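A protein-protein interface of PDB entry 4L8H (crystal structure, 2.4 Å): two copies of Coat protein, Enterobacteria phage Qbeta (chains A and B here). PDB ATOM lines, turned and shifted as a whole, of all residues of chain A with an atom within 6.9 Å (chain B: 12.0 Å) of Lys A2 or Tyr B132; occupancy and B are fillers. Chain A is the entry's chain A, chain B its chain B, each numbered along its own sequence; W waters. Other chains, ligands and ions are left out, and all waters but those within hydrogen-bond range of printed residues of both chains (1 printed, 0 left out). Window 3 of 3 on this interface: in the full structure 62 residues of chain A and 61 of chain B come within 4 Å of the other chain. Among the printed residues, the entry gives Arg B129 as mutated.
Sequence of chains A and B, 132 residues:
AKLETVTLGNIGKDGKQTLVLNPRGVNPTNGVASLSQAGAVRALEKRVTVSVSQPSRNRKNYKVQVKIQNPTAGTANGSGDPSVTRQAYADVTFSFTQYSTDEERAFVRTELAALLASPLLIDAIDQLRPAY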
ATOM      1  N   ALA A   1       7.892  29.666  15.723  1.00  0.00           N
ATOM      2  CA  ALA A   1       8.389  31.067  15.612  1.00  0.00           C
ATOM      3  C   ALA A   1       9.690  31.152  14.810  1.00  0.00           C
ATOM      4  O   ALA A   1      10.469  30.197  14.759  1.00  0.00           O
ATOM      5  CB  ALA A   1       8.559  31.702  17.003  1.00  0.00           C
ATOM      6  N   LYS A   2       9.881  32.300  14.160  1.00  0.00           N
ATOM      7  CA  LYS A   2      11.130  32.701  13.490  1.00  0.00           C
ATOM      8  C   LYS A   2      12.397  32.265  14.287  1.00  0.00           C
ATOM      9  O   LYS A   2      12.525  32.622  15.461  1.00  0.00           O
ATOM     10  CB  LYS A   2      11.083  34.243  13.289  1.00  0.00           C
ATOM     11  CG  LYS A   2      12.202  34.881  12.418  1.00  0.00           C
ATOM     12  CD  LYS A   2      12.165  34.421  10.955  1.00  0.00           C
ATOM     13  CE  LYS A   2      13.483  34.750  10.259  1.00  0.00           C
ATOM     14  NZ  LYS A   2      13.606  33.986   8.978  1.00  0.00           N
ATOM     15  N   LEU A   3      13.277  31.465  13.661  1.00  0.00           N
ATOM     16  CA  LEU A   3      14.603  31.098  14.225  1.00  0.00           C
ATOM     17  C   LEU A   3      15.373  32.328  14.699  1.00  0.00           C
ATOM     18  O   LEU A   3      15.602  33.259  13.935  1.00  0.00           O
ATOM     19  CB  LEU A   3      15.472  30.318  13.216  1.00  0.00           C
ATOM     20  CG  LEU A   3      16.778  29.744  13.797  1.00  0.00           C
ATOM     21  CD1 LEU A   3      16.490  28.676  14.852  1.00  0.00           C
ATOM     22  CD2 LEU A   3      17.722  29.176  12.757  1.00  0.00           C
ATOM     23  N   GLU A   4      15.775  32.309  15.960  1.00  0.00           N
ATOM     24  CA  GLU A   4      16.207  33.500  16.684  1.00  0.00           C
ATOM     25  C   GLU A   4      17.443  33.173  17.547  1.00  0.00           C
ATOM     26  O   GLU A   4      17.635  32.010  17.921  1.00  0.00           O
ATOM     27  CB  GLU A   4      15.046  33.935  17.576  1.00  0.00           C
ATOM     28  CG  GLU A   4      15.110  35.323  18.141  1.00  0.00           C
ATOM     29  CD  GLU A   4      14.044  35.558  19.212  1.00  0.00           C
ATOM     30  OE1 GLU A   4      13.728  34.617  19.993  1.00  0.00           O
ATOM     31  OE2 GLU A   4      13.524  36.701  19.286  1.00  0.00           O
ATOM     32  N   THR A   5      18.275  34.178  17.849  1.00  0.00           N
ATOM     33  CA  THR A   5      19.451  34.003  18.720  1.00  0.00           C
ATOM     34  C   THR A   5      19.074  33.366  20.064  1.00  0.00           C
ATOM     35  O   THR A   5      18.160  33.832  20.744  1.00  0.00           O
ATOM     36  CB  THR A   5      20.183  35.361  19.013  1.00  0.00           C
ATOM     37  OG1 THR A   5      20.945  35.728  17.878  1.00  0.00           O
ATOM     38  CG2 THR A   5      21.158  35.253  20.196  1.00  0.00           C
ATOM     39  N   GLY A  25      19.956  29.406   9.822  1.00  0.00           N
ATOM     40  CA  GLY A  25      18.937  29.064   8.849  1.00  0.00           C
ATOM     41  C   GLY A  25      18.273  27.721   9.045  1.00  0.00           C
ATOM     42  O   GLY A  25      18.831  26.794   9.653  1.00  0.00           O
ATOM     43  N   VAL A  26      17.058  27.634   8.519  1.00  0.00           N
ATOM     44  CA  VAL A  26      16.307  26.411   8.497  1.00  0.00           C
ATOM     45  C   VAL A  26      16.581  25.818   7.137  1.00  0.00           C
ATOM     46  O   VAL A  26      16.674  26.537   6.151  1.00  0.00           O
ATOM     47  CB  VAL A  26      14.821  26.708   8.718  1.00  0.00           C
ATOM     48  CG1 VAL A  26      13.965  25.446   8.593  1.00  0.00           C
ATOM     49  CG2 VAL A  26      14.624  27.388  10.095  1.00  0.00           C
ATOM     50  N   ALA A  33      16.610  23.153  11.804  1.00  0.00           N
ATOM     51  CA  ALA A  33      17.058  24.458  12.194  1.00  0.00           C
ATOM     52  C   ALA A  33      18.486  24.349  12.735  1.00  0.00           C
ATOM     53  O   ALA A  33      18.748  23.526  13.584  1.00  0.00           O
ATOM     54  CB  ALA A  33      16.124  25.003  13.253  1.00  0.00           C
ATOM     55  N   SER B 118      14.950  26.953  26.894  1.00  0.00           N
ATOM     56  CA  SER B 118      14.872  28.058  25.967  1.00  0.00           C
ATOM     57  C   SER B 118      13.530  28.112  25.181  1.00  0.00           C
ATOM     58  O   SER B 118      12.920  27.061  24.887  1.00  0.00           O
ATOM     59  CB  SER B 118      16.033  27.986  24.999  1.00  0.00           C
ATOM     60  OG  SER B 118      15.792  26.997  24.035  1.00  0.00           O
ATOM     61  N   PRO B 119      13.087  29.342  24.813  1.00  0.00           N
ATOM     62  CA  PRO B 119      11.845  29.521  24.020  1.00  0.00           C
ATOM     63  C   PRO B 119      11.899  28.619  22.814  1.00  0.00           C
ATOM     64  O   PRO B 119      10.866  28.084  22.391  1.00  0.00           O
ATOM     65  CB  PRO B 119      11.924  31.009  23.574  1.00  0.00           C
ATOM     66  CG  PRO B 119      12.644  31.678  24.767  1.00  0.00           C
ATOM     67  CD  PRO B 119      13.718  30.649  25.135  1.00  0.00           C
ATOM     68  N   LEU B 120      13.096  28.412  22.276  1.00  0.00           N
ATOM     69  CA  LEU B 120      13.186  27.605  21.072  1.00  0.00           C
ATOM     70  C   LEU B 120      12.730  26.157  21.345  1.00  0.00           C
ATOM     71  O   LEU B 120      12.058  25.556  20.515  1.00  0.00           O
ATOM     72  CB  LEU B 120      14.583  27.653  20.427  1.00  0.00           C
ATOM     73  CG  LEU B 120      14.725  26.645  19.298  1.00  0.00           C
ATOM     74  CD1 LEU B 120      13.811  26.966  18.125  1.00  0.00           C
ATOM     75  CD2 LEU B 120      16.164  26.534  18.841  1.00  0.00           C
ATOM     76  N   LEU B 121      13.079  25.623  22.516  1.00  0.00           N
ATOM     77  CA  LEU B 121      12.792  24.233  22.828  1.00  0.00           C
ATOM     78  C   LEU B 121      11.432  24.032  23.503  1.00  0.00           C
ATOM     79  O   LEU B 121      10.847  22.973  23.379  1.00  0.00           O
ATOM     80  CB  LEU B 121      13.929  23.612  23.654  1.00  0.00           C
ATOM     81  CG  LEU B 121      14.827  22.638  22.890  1.00  0.00           C
ATOM     82  CD1 LEU B 121      15.318  23.174  21.632  1.00  0.00           C
ATOM     83  CD2 LEU B 121      15.990  22.356  23.721  1.00  0.00           C
ATOM     84  N   ILE B 122      10.950  25.046  24.207  1.00  0.00           N
ATOM     85  CA  ILE B 122       9.574  25.066  24.670  1.00  0.00           C
ATOM     86  C   ILE B 122       8.559  24.965  23.466  1.00  0.00           C
ATOM     87  O   ILE B 122       7.526  24.279  23.573  1.00  0.00           O
ATOM     88  CB  ILE B 122       9.313  26.299  25.582  1.00  0.00           C
ATOM     89  CG1 ILE B 122      10.172  26.215  26.859  1.00  0.00           C
ATOM     90  CG2 ILE B 122       7.845  26.466  25.899  1.00  0.00           C
ATOM     91  CD1 ILE B 122      10.169  27.483  27.796  1.00  0.00           C
ATOM     92  N   ASP B 123       8.872  25.594  22.330  1.00  0.00           N
ATOM     93  CA  ASP B 123       7.925  25.631  21.221  1.00  0.00           C
ATOM     94  C   ASP B 123       7.949  24.330  20.501  1.00  0.00           C
ATOM     95  O   ASP B 123       6.898  23.846  20.055  1.00  0.00           O
ATOM     96  CB  ASP B 123       8.251  26.715  20.181  1.00  0.00           C
ATOM     97  CG  ASP B 123       8.105  28.110  20.720  1.00  0.00           C
ATOM     98  OD1 ASP B 123       7.376  28.294  21.729  1.00  0.00           O
ATOM     99  OD2 ASP B 123       8.752  29.032  20.145  1.00  0.00           O
ATOM    100  N   ALA B 124       9.174  23.818  20.322  1.00  0.00           N
ATOM    101  CA  ALA B 124       9.386  22.560  19.607  1.00  0.00           C
ATOM    102  C   ALA B 124       8.755  21.406  20.372  1.00  0.00           C
ATOM    103  O   ALA B 124       8.110  20.553  19.753  1.00  0.00           O
ATOM    104  CB  ALA B 124      10.854  22.310  19.391  1.00  0.00           C
ATOM    105  N   GLN B 127       4.690  22.893  22.549  1.00  0.00           N
ATOM    106  CA  GLN B 127       3.769  23.236  21.483  1.00  0.00           C
ATOM    107  C   GLN B 127       3.994  22.471  20.188  1.00  0.00           C
ATOM    108  O   GLN B 127       3.213  22.624  19.271  1.00  0.00           O
ATOM    109  CB  GLN B 127       3.845  24.726  21.179  1.00  0.00           C
ATOM    110  CG  GLN B 127       2.843  25.515  21.929  1.00  0.00           C
ATOM    111  CD  GLN B 127       3.093  25.474  23.410  1.00  0.00           C
ATOM    112  OE1 GLN B 127       2.331  24.842  24.172  1.00  0.00           O
ATOM    113  NE2 GLN B 127       4.173  26.149  23.847  1.00  0.00           N
ATOM    114  N   LEU B 128       5.040  21.659  20.074  1.00  0.00           N
ATOM    115  CA  LEU B 128       5.260  20.985  18.785  1.00  0.00           C
ATOM    116  C   LEU B 128       5.361  21.968  17.555  1.00  0.00           C
ATOM    117  O   LEU B 128       4.988  21.634  16.429  1.00  0.00           O
ATOM    118  CB  LEU B 128       4.222  19.868  18.553  1.00  0.00           C
ATOM    119  CG  LEU B 128       4.379  18.613  19.459  1.00  0.00           C
ATOM    120  CD1 LEU B 128       3.105  17.736  19.492  1.00  0.00           C
ATOM    121  CD2 LEU B 128       5.646  17.710  19.157  1.00  0.00           C
ATOM    122  N   ARG B 129       5.903  23.161  17.780  1.00  0.00           N
ATOM    123  CA  ARG B 129       6.108  24.129  16.689  1.00  0.00           C
ATOM    124  C   ARG B 129       7.570  24.306  16.241  1.00  0.00           C
ATOM    125  O   ARG B 129       8.430  24.750  17.018  1.00  0.00           O
ATOM    126  CB  ARG B 129       5.457  25.481  17.013  1.00  0.00           C
ATOM    127  CG  ARG B 129       3.937  25.468  16.872  1.00  0.00           C
ATOM    128  CD  ARG B 129       3.281  26.679  17.567  1.00  0.00           C
ATOM    129  NE  ARG B 129       1.929  26.335  18.059  1.00  0.00           N
ATOM    130  CZ  ARG B 129       1.266  27.001  19.012  1.00  0.00           C
ATOM    131  NH1 ARG B 129       1.814  28.063  19.606  1.00  0.00           N
ATOM    132  NH2 ARG B 129       0.064  26.582  19.395  1.00  0.00           N
ATOM    133  N   PRO B 130       7.862  23.935  14.982  1.00  0.00           N
ATOM    134  CA  PRO B 130       9.204  24.218  14.437  1.00  0.00           C
ATOM    135  C   PRO B 130       9.511  25.705  14.340  1.00  0.00           C
ATOM    136  O   PRO B 130       8.610  26.534  14.212  1.00  0.00           O
ATOM    137  CB  PRO B 130       9.175  23.603  13.039  1.00  0.00           C
ATOM    138  CG  PRO B 130       7.695  23.420  12.703  1.00  0.00           C
ATOM    139  CD  PRO B 130       7.016  23.185  14.035  1.00  0.00           C
ATOM    140  N   ALA B 131      10.795  26.036  14.456  1.00  0.00           N
ATOM    141  CA  ALA B 131      11.268  27.357  14.100  1.00  0.00           C
ATOM    142  C   ALA B 131      11.321  27.447  12.563  1.00  0.00           C
ATOM    143  O   ALA B 131      11.488  26.428  11.876  1.00  0.00           O
ATOM    144  CB  ALA B 131      12.632  27.607  14.699  1.00  0.00           C
ATOM    145  N   TYR B 132      11.156  28.650  12.026  1.00  0.00           N
ATOM    146  CA  TYR B 132      11.334  28.842  10.585  1.00  0.00           C
ATOM    147  C   TYR B 132      12.359  29.945  10.279  1.00  0.00           C
ATOM    148  O   TYR B 132      12.773  30.753  11.104  1.00  0.00           O
ATOM    149  CB  TYR B 132       9.988  29.066   9.865  1.00  0.00           C
ATOM    150  CG  TYR B 132       9.035  29.895  10.682  1.00  0.00           C
ATOM    151  CD1 TYR B 132       9.093  31.296  10.655  1.00  0.00           C
ATOM    152  CD2 TYR B 132       8.110  29.278  11.528  1.00  0.00           C
ATOM    153  CE1 TYR B 132       8.252  32.056  11.434  1.00  0.00           C
ATOM    154  CE2 TYR B 132       7.257  30.029  12.318  1.00  0.00           C
ATOM    155  CZ  TYR B 132       7.330  31.417  12.263  1.00  0.00           C
ATOM    156  OH  TYR B 132       6.466  32.150  13.042  1.00  0.00           O
ATOM    157  OXT TYR B 132      12.847  30.043   9.171  1.00  0.00           O
HETATM  158  O   HOH W   1      14.823  31.697   9.355  1.00  0.00           O
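The backbone NH of Leu A3 lies within hydrogen-bond range of the chain-end carboxylate of Tyr B132 (2.7 Å).
O of Ala A1 lies within hydrogen-bond range of N of Tyr B132 (3.2 Å).
The chain-end carboxylate of Tyr B132 is in salt-bridge range of the side-chain amino group of Lys A2 (3.96 Å).
Among the printed residues, pairs that only touch across the chains: Ala A1 with Ala B131 (3.0 Å), Val A26 with Tyr B132 (3.3 Å), Ala A1 with Pro B130 (3.6 Å) and Val A26 with Ala B131 (3.7 Å).
Ala A1 touches just these residues of chain B: Pro B130 (3.6 Å), Ala B131 (3.0 Å) and Tyr B132 (3.2 Å).
Of chain B, only Tyr B132 comes within 4 Å of Lys A2.
Printed residues of chain B within 4 Å of Leu A3: Tyr B132.
No residue of chain B comes within 4 Å of Glu A4.
Thr A5 touches none of the printed residues of chain B.
Ala B124 touches none of the printed residues of chain A.
Of the printed residues of chain A, Pro B130 touches Ala A1.
Of the printed residues of chain A, Ala B131 touches Ala A1 and Val A26.
Of the printed residues of chain A, Tyr B132 touches Ala A1, Lys A2, Leu A3 and Val A26.
The nearest residue of chain B that does not touch Lys A2 is Ala B131 (4.7 Å).
The nearest printed residue of chain A that does not touch Tyr B132 is Gly A25 (5.9 Å).
The nearest printed residue of chain A that does not touch Ala B131 is Leu A3 (4.01 Å).
Hydrophobic or aromatic side chains of chain A that line the printed part of chain B: Leu A3 and Val A26.
Of the 13 printed residues of chain B, 3 touch a printed residue of chain A.
Hydrophobic or aromatic side chains of chain B within 4 Å of the printed part of chain A: Ala B131 and Tyr B132.
Among the printed residues, 7 pairs touch across the chains.
Among the printed residues, no Asp or Glu carboxylate lies within 4 Å of a Lys or Arg side-chain nitrogen of the other chain.
No position is printed for both chains.
Of the 7 pairs that touch across the chains among the printed residues, none has its exchanged pair printed and touching as well.
Water W1 bridges OXT of Tyr B132 (2.6 Å) and NZ of Lys A2 (2.6 Å).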
